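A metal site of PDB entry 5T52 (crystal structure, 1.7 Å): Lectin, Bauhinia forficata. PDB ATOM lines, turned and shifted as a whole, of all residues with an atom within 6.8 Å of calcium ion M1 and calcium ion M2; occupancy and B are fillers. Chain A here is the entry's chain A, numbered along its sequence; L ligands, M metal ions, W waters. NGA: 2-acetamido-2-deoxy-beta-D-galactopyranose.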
ATOM      1  N   ASP A  78     -10.450  27.513  16.843  1.00  0.00           N
ATOM      2  CA  ASP A  78      -9.746  26.340  16.293  1.00  0.00           C
ATOM      3  C   ASP A  78      -8.595  26.693  15.457  1.00  0.00           C
ATOM      4  O   ASP A  78      -7.771  25.838  15.186  1.00  0.00           O
ATOM      5  CB  ASP A  78     -10.679  25.433  15.457  1.00  0.00           C
ATOM      6  CG  ASP A  78     -11.504  24.573  16.364  1.00  0.00           C
ATOM      7  OD1 ASP A  78     -10.980  23.480  16.752  1.00  0.00           O
ATOM      8  OD2 ASP A  78     -12.655  24.952  16.786  1.00  0.00           O
ATOM      9  N   GLY A  95     -15.589  24.577  13.996  1.00  0.00           N
ATOM     10  CA  GLY A  95     -14.845  23.758  14.903  1.00  0.00           C
ATOM     11  C   GLY A  95     -13.562  23.294  14.234  1.00  0.00           C
ATOM     12  O   GLY A  95     -12.988  24.015  13.425  1.00  0.00           O
ATOM     13  N   GLY A  96     -13.129  22.091  14.556  1.00  0.00           N
ATOM     14  CA  GLY A  96     -11.832  21.607  14.089  1.00  0.00           C
ATOM     15  C   GLY A  96     -11.730  21.331  12.627  1.00  0.00           C
ATOM     16  O   GLY A  96     -10.598  21.167  12.107  1.00  0.00           O
ATOM     17  N   TYR A  97     -12.882  21.395  11.927  1.00  0.00           N
ATOM     18  CA  TYR A  97     -12.879  21.248  10.456  1.00  0.00           C
ATOM     19  C   TYR A  97     -12.425  22.549   9.748  1.00  0.00           C
ATOM     20  O   TYR A  97     -12.179  22.540   8.520  1.00  0.00           O
ATOM     21  CB  TYR A  97     -14.250  20.831   9.988  1.00  0.00           C
ATOM     22  CG  TYR A  97     -14.679  19.554  10.611  1.00  0.00           C
ATOM     23  CD1 TYR A  97     -14.128  18.329  10.192  1.00  0.00           C
ATOM     24  CD2 TYR A  97     -15.644  19.553  11.632  1.00  0.00           C
ATOM     25  CE1 TYR A  97     -14.498  17.108  10.817  1.00  0.00           C
ATOM     26  CE2 TYR A  97     -16.004  18.394  12.205  1.00  0.00           C
ATOM     27  CZ  TYR A  97     -15.451  17.181  11.807  1.00  0.00           C
ATOM     28  OH  TYR A  97     -15.893  15.996  12.424  1.00  0.00           O
ATOM     29  N   LEU A  98     -12.264  23.658  10.510  1.00  0.00           N
ATOM     30  CA  LEU A  98     -11.617  24.864  10.081  1.00  0.00           C
ATOM     31  C   LEU A  98     -12.415  25.547   8.984  1.00  0.00           C
ATOM     32  O   LEU A  98     -11.864  26.317   8.221  1.00  0.00           O
ATOM     33  CB  LEU A  98     -10.119  24.668   9.682  1.00  0.00           C
ATOM     34  CG  LEU A  98      -9.270  24.220  10.899  1.00  0.00           C
ATOM     35  CD1 LEU A  98      -7.865  23.971  10.423  1.00  0.00           C
ATOM     36  CD2 LEU A  98      -9.250  25.295  11.970  1.00  0.00           C
ATOM     37  N   GLU A 118      -2.586  25.437   7.301  1.00  0.00           N
ATOM     38  CA  GLU A 118      -3.450  25.653   8.434  1.00  0.00           C
ATOM     39  C   GLU A 118      -2.597  26.035   9.708  1.00  0.00           C
ATOM     40  O   GLU A 118      -1.418  25.641   9.823  1.00  0.00           O
ATOM     41  CB  GLU A 118      -4.291  24.391   8.684  1.00  0.00           C
ATOM     42  CG  GLU A 118      -3.471  23.220   9.267  1.00  0.00           C
ATOM     43  CD  GLU A 118      -4.279  22.112   9.861  1.00  0.00           C
ATOM     44  OE1 GLU A 118      -5.285  21.629   9.281  1.00  0.00           O
ATOM     45  OE2 GLU A 118      -3.874  21.635  10.947  1.00  0.00           O
ATOM     46  N   ASP A 120      -3.196  25.791  13.520  1.00  0.00           N
ATOM     47  CA  ASP A 120      -4.150  25.031  14.267  1.00  0.00           C
ATOM     48  C   ASP A 120      -3.925  25.218  15.721  1.00  0.00           C
ATOM     49  O   ASP A 120      -2.936  24.745  16.263  1.00  0.00           O
ATOM     50  CB  ASP A 120      -4.043  23.494  13.879  1.00  0.00           C
ATOM     51  CG  ASP A 120      -5.146  22.591  14.471  1.00  0.00           C
ATOM     52  OD1 ASP A 120      -5.774  22.968  15.474  1.00  0.00           O
ATOM     53  OD2 ASP A 120      -5.487  21.522  13.840  1.00  0.00           O
ATOM     54  N   THR A 121      -4.898  25.935  16.413  1.00  0.00           N
ATOM     55  CA  THR A 121      -4.775  26.222  17.838  1.00  0.00           C
ATOM     56  C   THR A 121      -5.342  25.208  18.812  1.00  0.00           C
ATOM     57  O   THR A 121      -5.167  25.349  20.008  1.00  0.00           O
ATOM     58  CB  THR A 121      -5.415  27.553  18.138  1.00  0.00           C
ATOM     59  OG1 THR A 121      -6.785  27.409  17.798  1.00  0.00           O
ATOM     60  CG2 THR A 121      -4.742  28.622  17.405  1.00  0.00           C
ATOM     61  N   TRP A 122      -6.042  24.199  18.273  1.00  0.00           N
ATOM     62  CA  TRP A 122      -6.788  23.265  19.120  1.00  0.00           C
ATOM     63  C   TRP A 122      -6.478  21.821  18.725  1.00  0.00           C
ATOM     64  O   TRP A 122      -6.789  21.371  17.652  1.00  0.00           O
ATOM     65  CB  TRP A 122      -8.315  23.526  19.058  1.00  0.00           C
ATOM     66  CG  TRP A 122      -9.098  22.543  19.847  1.00  0.00           C
ATOM     67  CD1 TRP A 122      -9.526  21.301  19.416  1.00  0.00           C
ATOM     68  CD2 TRP A 122      -9.520  22.677  21.187  1.00  0.00           C
ATOM     69  NE1 TRP A 122     -10.202  20.658  20.453  1.00  0.00           N
ATOM     70  CE2 TRP A 122     -10.244  21.521  21.528  1.00  0.00           C
ATOM     71  CE3 TRP A 122      -9.387  23.704  22.149  1.00  0.00           C
ATOM     72  CZ2 TRP A 122     -10.729  21.324  22.816  1.00  0.00           C
ATOM     73  CZ3 TRP A 122      -9.929  23.506  23.382  1.00  0.00           C
ATOM     74  CH2 TRP A 122     -10.621  22.359  23.690  1.00  0.00           C
ATOM     75  N   VAL A 123      -5.899  21.066  19.656  1.00  0.00           N
ATOM     76  CA  VAL A 123      -5.541  19.723  19.338  1.00  0.00           C
ATOM     77  C   VAL A 123      -6.856  18.895  19.359  1.00  0.00           C
ATOM     78  O   VAL A 123      -7.463  18.734  20.477  1.00  0.00           O
ATOM     79  CB  VAL A 123      -4.579  19.173  20.422  1.00  0.00           C
ATOM     80  CG1 VAL A 123      -4.358  17.670  20.192  1.00  0.00           C
ATOM     81  CG2 VAL A 123      -3.242  19.904  20.323  1.00  0.00           C
ATOM     82  N   ASN A 124      -7.189  18.266  18.272  1.00  0.00           N
ATOM     83  CA  ASN A 124      -8.355  17.410  18.131  1.00  0.00           C
ATOM     84  C   ASN A 124      -7.973  15.957  18.297  1.00  0.00           C
ATOM     85  O   ASN A 124      -6.940  15.526  17.810  1.00  0.00           O
ATOM     86  CB  ASN A 124      -8.934  17.599  16.731  1.00  0.00           C
ATOM     87  CG  ASN A 124      -9.668  18.911  16.588  1.00  0.00           C
ATOM     88  OD1 ASN A 124      -9.151  19.893  16.003  1.00  0.00           O
ATOM     89  ND2 ASN A 124     -10.945  18.920  17.046  1.00  0.00           N
ATOM     90  N   TRP A 127      -9.649  12.976  15.245  1.00  0.00           N
ATOM     91  CA  TRP A 127      -8.815  12.423  14.184  1.00  0.00           C
ATOM     92  C   TRP A 127      -7.376  12.568  14.572  1.00  0.00           C
ATOM     93  O   TRP A 127      -7.073  13.177  15.593  1.00  0.00           O
ATOM     94  CB  TRP A 127      -9.109  13.116  12.827  1.00  0.00           C
ATOM     95  CG  TRP A 127      -9.012  14.644  12.914  1.00  0.00           C
ATOM     96  CD1 TRP A 127      -7.880  15.437  12.921  1.00  0.00           C
ATOM     97  CD2 TRP A 127     -10.128  15.530  13.072  1.00  0.00           C
ATOM     98  NE1 TRP A 127      -8.235  16.750  13.099  1.00  0.00           N
ATOM     99  CE2 TRP A 127      -9.617  16.836  13.201  1.00  0.00           C
ATOM    100  CE3 TRP A 127     -11.501  15.313  13.241  1.00  0.00           C
ATOM    101  CZ2 TRP A 127     -10.442  17.956  13.324  1.00  0.00           C
ATOM    102  CZ3 TRP A 127     -12.355  16.460  13.331  1.00  0.00           C
ATOM    103  CH2 TRP A 127     -11.788  17.754  13.466  1.00  0.00           C
ATOM    104  N   LYS A 128      -6.463  12.059  13.730  1.00  0.00           N
ATOM    105  CA  LYS A 128      -5.025  12.085  14.060  1.00  0.00           C
ATOM    106  C   LYS A 128      -4.416  13.457  13.819  1.00  0.00           C
ATOM    107  O   LYS A 128      -4.516  14.019  12.728  1.00  0.00           O
ATOM    108  CB  LYS A 128      -4.257  11.054  13.246  1.00  0.00           C
ATOM    109  CG  LYS A 128      -4.560   9.608  13.669  1.00  0.00           C
ATOM    110  CD  LYS A 128      -3.642   8.520  13.048  1.00  0.00           C
ATOM    111  CE  LYS A 128      -3.919   7.096  13.593  1.00  0.00           C
ATOM    112  NZ  LYS A 128      -3.284   5.913  12.895  1.00  0.00           N
ATOM    113  N   GLU A 129      -3.913  14.052  14.887  1.00  0.00           N
ATOM    114  CA  GLU A 129      -3.031  15.208  14.738  1.00  0.00           C
ATOM    115  C   GLU A 129      -2.149  15.306  15.903  1.00  0.00           C
ATOM    116  O   GLU A 129      -2.295  14.529  16.853  1.00  0.00           O
ATOM    117  CB  GLU A 129      -3.756  16.504  14.399  1.00  0.00           C
ATOM    118  CG  GLU A 129      -4.886  16.915  15.354  1.00  0.00           C
ATOM    119  CD  GLU A 129      -5.612  18.255  14.941  1.00  0.00           C
ATOM    120  OE1 GLU A 129      -5.785  18.541  13.738  1.00  0.00           O
ATOM    121  OE2 GLU A 129      -6.007  19.014  15.833  1.00  0.00           O
ATOM    122  N   PRO A 130      -1.126  16.160  15.804  1.00  0.00           N
ATOM    123  CA  PRO A 130      -0.182  16.155  16.894  1.00  0.00           C
ATOM    124  C   PRO A 130      -0.715  16.615  18.229  1.00  0.00           C
ATOM    125  O   PRO A 130      -1.706  17.269  18.310  1.00  0.00           O
ATOM    126  CB  PRO A 130       0.927  17.146  16.440  1.00  0.00           C
ATOM    127  CG  PRO A 130       0.697  17.415  14.962  1.00  0.00           C
ATOM    128  CD  PRO A 130      -0.735  17.104  14.725  1.00  0.00           C
ATOM    129  N   HIS A 134      -0.045  23.398  16.101  1.00  0.00           N
ATOM    130  CA  HIS A 134       0.783  23.056  14.972  1.00  0.00           C
ATOM    131  C   HIS A 134       0.362  23.835  13.770  1.00  0.00           C
ATOM    132  O   HIS A 134      -0.744  24.277  13.724  1.00  0.00           O
ATOM    133  CB  HIS A 134       0.767  21.526  14.772  1.00  0.00           C
ATOM    134  CG  HIS A 134      -0.617  20.941  14.617  1.00  0.00           C
ATOM    135  ND1 HIS A 134      -1.417  20.690  15.701  1.00  0.00           N
ATOM    136  CD2 HIS A 134      -1.413  20.780  13.528  1.00  0.00           C
ATOM    137  CE1 HIS A 134      -2.597  20.254  15.295  1.00  0.00           C
ATOM    138  NE2 HIS A 134      -2.627  20.284  13.989  1.00  0.00           N
ATOM    139  N   GLY A 136       0.400  23.245   9.538  1.00  0.00           N
ATOM    140  CA  GLY A 136       0.286  22.095   8.662  1.00  0.00           C
ATOM    141  C   GLY A 136      -0.002  22.427   7.253  1.00  0.00           C
ATOM    142  O   GLY A 136      -0.582  23.451   6.969  1.00  0.00           O
ATOM    143  N   ASP A 138      -2.331  20.793   4.335  1.00  0.00           N
ATOM    144  CA  ASP A 138      -3.439  19.857   4.138  1.00  0.00           C
ATOM    145  C   ASP A 138      -3.691  19.672   2.710  1.00  0.00           C
ATOM    146  O   ASP A 138      -3.849  20.667   1.940  1.00  0.00           O
ATOM    147  CB  ASP A 138      -4.705  20.479   4.743  1.00  0.00           C
ATOM    148  CG  ASP A 138      -4.587  20.747   6.262  1.00  0.00           C
ATOM    149  OD1 ASP A 138      -3.728  20.134   6.942  1.00  0.00           O
ATOM    150  OD2 ASP A 138      -5.446  21.542   6.818  1.00  0.00           O
ATOM    151  N   ILE A 142      -8.456  16.840   6.433  1.00  0.00           N
ATOM    152  CA  ILE A 142      -8.161  17.565   7.695  1.00  0.00           C
ATOM    153  C   ILE A 142      -6.972  16.990   8.496  1.00  0.00           C
ATOM    154  O   ILE A 142      -6.348  17.693   9.342  1.00  0.00           O
ATOM    155  CB  ILE A 142      -9.415  17.607   8.623  1.00  0.00           C
ATOM    156  CG1 ILE A 142      -9.314  18.761   9.675  1.00  0.00           C
ATOM    157  CG2 ILE A 142      -9.679  16.246   9.258  1.00  0.00           C
ATOM    158  CD1 ILE A 142      -9.073  20.195   9.218  1.00  0.00           C
ATOM    159  N   VAL A 143      -6.546  15.804   8.105  1.00  0.00           N
ATOM    160  CA  VAL A 143      -5.323  15.199   8.661  1.00  0.00           C
ATOM    161  C   VAL A 143      -4.136  15.646   7.774  1.00  0.00           C
ATOM    162  O   VAL A 143      -3.981  15.250   6.607  1.00  0.00           O
ATOM    163  CB  VAL A 143      -5.398  13.643   8.727  1.00  0.00           C
ATOM    164  CG1 VAL A 143      -4.131  13.083   9.271  1.00  0.00           C
ATOM    165  CG2 VAL A 143      -6.519  13.273   9.681  1.00  0.00           C
ATOM    166  N   SER A 144      -3.334  16.560   8.306  1.00  0.00           N
ATOM    167  CA  SER A 144      -2.274  17.153   7.499  1.00  0.00           C
ATOM    168  C   SER A 144      -1.285  16.162   7.008  1.00  0.00           C
ATOM    169  O   SER A 144      -0.863  15.261   7.733  1.00  0.00           O
ATOM    170  CB  SER A 144      -1.492  18.214   8.313  1.00  0.00           C
ATOM    171  OG  SER A 144      -2.367  19.186   8.936  1.00  0.00           O
ATOM    172  N   VAL A 147       3.330  18.440   9.037  1.00  0.00           N
ATOM    173  CA  VAL A 147       2.958  19.212  10.201  1.00  0.00           C
ATOM    174  C   VAL A 147       4.197  19.545  11.016  1.00  0.00           C
ATOM    175  O   VAL A 147       5.159  18.803  11.001  1.00  0.00           O
ATOM    176  CB  VAL A 147       1.854  18.386  10.952  1.00  0.00           C
ATOM    177  CG1 VAL A 147       2.414  17.199  11.804  1.00  0.00           C
ATOM    178  CG2 VAL A 147       1.053  19.328  11.704  1.00  0.00           C
HETATM  179  C1  NGA L   1     -15.017  20.427  19.878  1.00  0.00           C
HETATM  180  C2  NGA L   1     -14.455  20.644  18.469  1.00  0.00           C
HETATM  181  C3  NGA L   1     -13.053  21.195  18.513  1.00  0.00           C
HETATM  182  C4  NGA L   1     -13.066  22.523  19.297  1.00  0.00           C
HETATM  183  C5  NGA L   1     -13.785  22.224  20.611  1.00  0.00           C
HETATM  184  C6  NGA L   1     -13.929  23.493  21.421  1.00  0.00           C
HETATM  185  C7  NGA L   1     -14.738  19.269  16.451  1.00  0.00           C
HETATM  186  C8  NGA L   1     -14.717  17.936  15.803  1.00  0.00           C
HETATM  187  N2  NGA L   1     -14.438  19.363  17.704  1.00  0.00           N
HETATM  188  O1  NGA L   1     -16.343  19.995  19.835  1.00  0.00           O
HETATM  189  O3  NGA L   1     -12.452  21.291  17.234  1.00  0.00           O
HETATM  190  O4  NGA L   1     -13.821  23.485  18.588  1.00  0.00           O
HETATM  191  O5  NGA L   1     -15.098  21.704  20.538  1.00  0.00           O
HETATM  192  O6  NGA L   1     -14.585  23.300  22.693  1.00  0.00           O
HETATM  193  O7  NGA L   1     -15.056  20.226  15.761  1.00  0.00           O
HETATM  194 CA    CA M   1      -4.546  20.054  12.445  1.00  0.00          CA
HETATM  195 CA    CA M   2      -7.278  21.057  15.348  1.00  0.00          CA
HETATM  196  O   HOH W   1      -3.343  18.548  11.353  1.00  0.00           O
HETATM  197  O   HOH W   2      -8.689  23.032  15.394  1.00  0.00           O
HETATM  198  O   HOH W   3      -6.409  19.970  10.940  1.00  0.00           O
HETATM  199  O   HOH W   4      -8.182  20.615  13.168  1.00  0.00           O
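O3 of the ligand sits at hydrogen-bond distance from ND2 of Asn 124. The backbone NH (N) of Gly 96 sits at hydrogen-bond distance from an oxygen (O3) of the ligand. The side-chain carboxylate (OD2) of Asp 78 lies within hydrogen-bond range of an oxygen (O4) of the ligand (2.6 Å).
OD2 of Asp 138 sits close to OE1 of Glu 118 (2.5 Å). N of Glu 118 is in hydrogen-bond range of O of Gly 136, 2.8 Å away. The side-chain carboxylate (OE1) of Glu 129 sits close to the indole nitrogen (NE1) of Trp 127, 3.1 Å away.
Within 4 Å of calcium ion M1: Glu 118, Asp 120, Glu 129 and His 134.
Calcium ion M1 is bound by water W1, the side-chain carboxylate of Asp 120, the side-chain carboxylate of Glu 118, the side-chain carboxylate of Glu 129, water W3 and a ring nitrogen (NE2) of His 134.
Calcium ion M2 is bound by the side-chain amide oxygen (OD1) of Asn 124, the backbone carbonyl oxygen (O) of Trp 122, the side-chain carboxylate (OD2) of Asp 120, water W4, water W2, the side-chain carboxylate (OD1) of Asp 120 and the side-chain carboxylate (OE2) of Glu 129. Calcium ion M2 has seven donor atoms within binding distance.
Water W3 lies within hydrogen-bond range of the side-chain carboxylate of Glu 118 (2.6 Å) and the backbone carbonyl oxygen of Ile 142 (2.8 Å).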
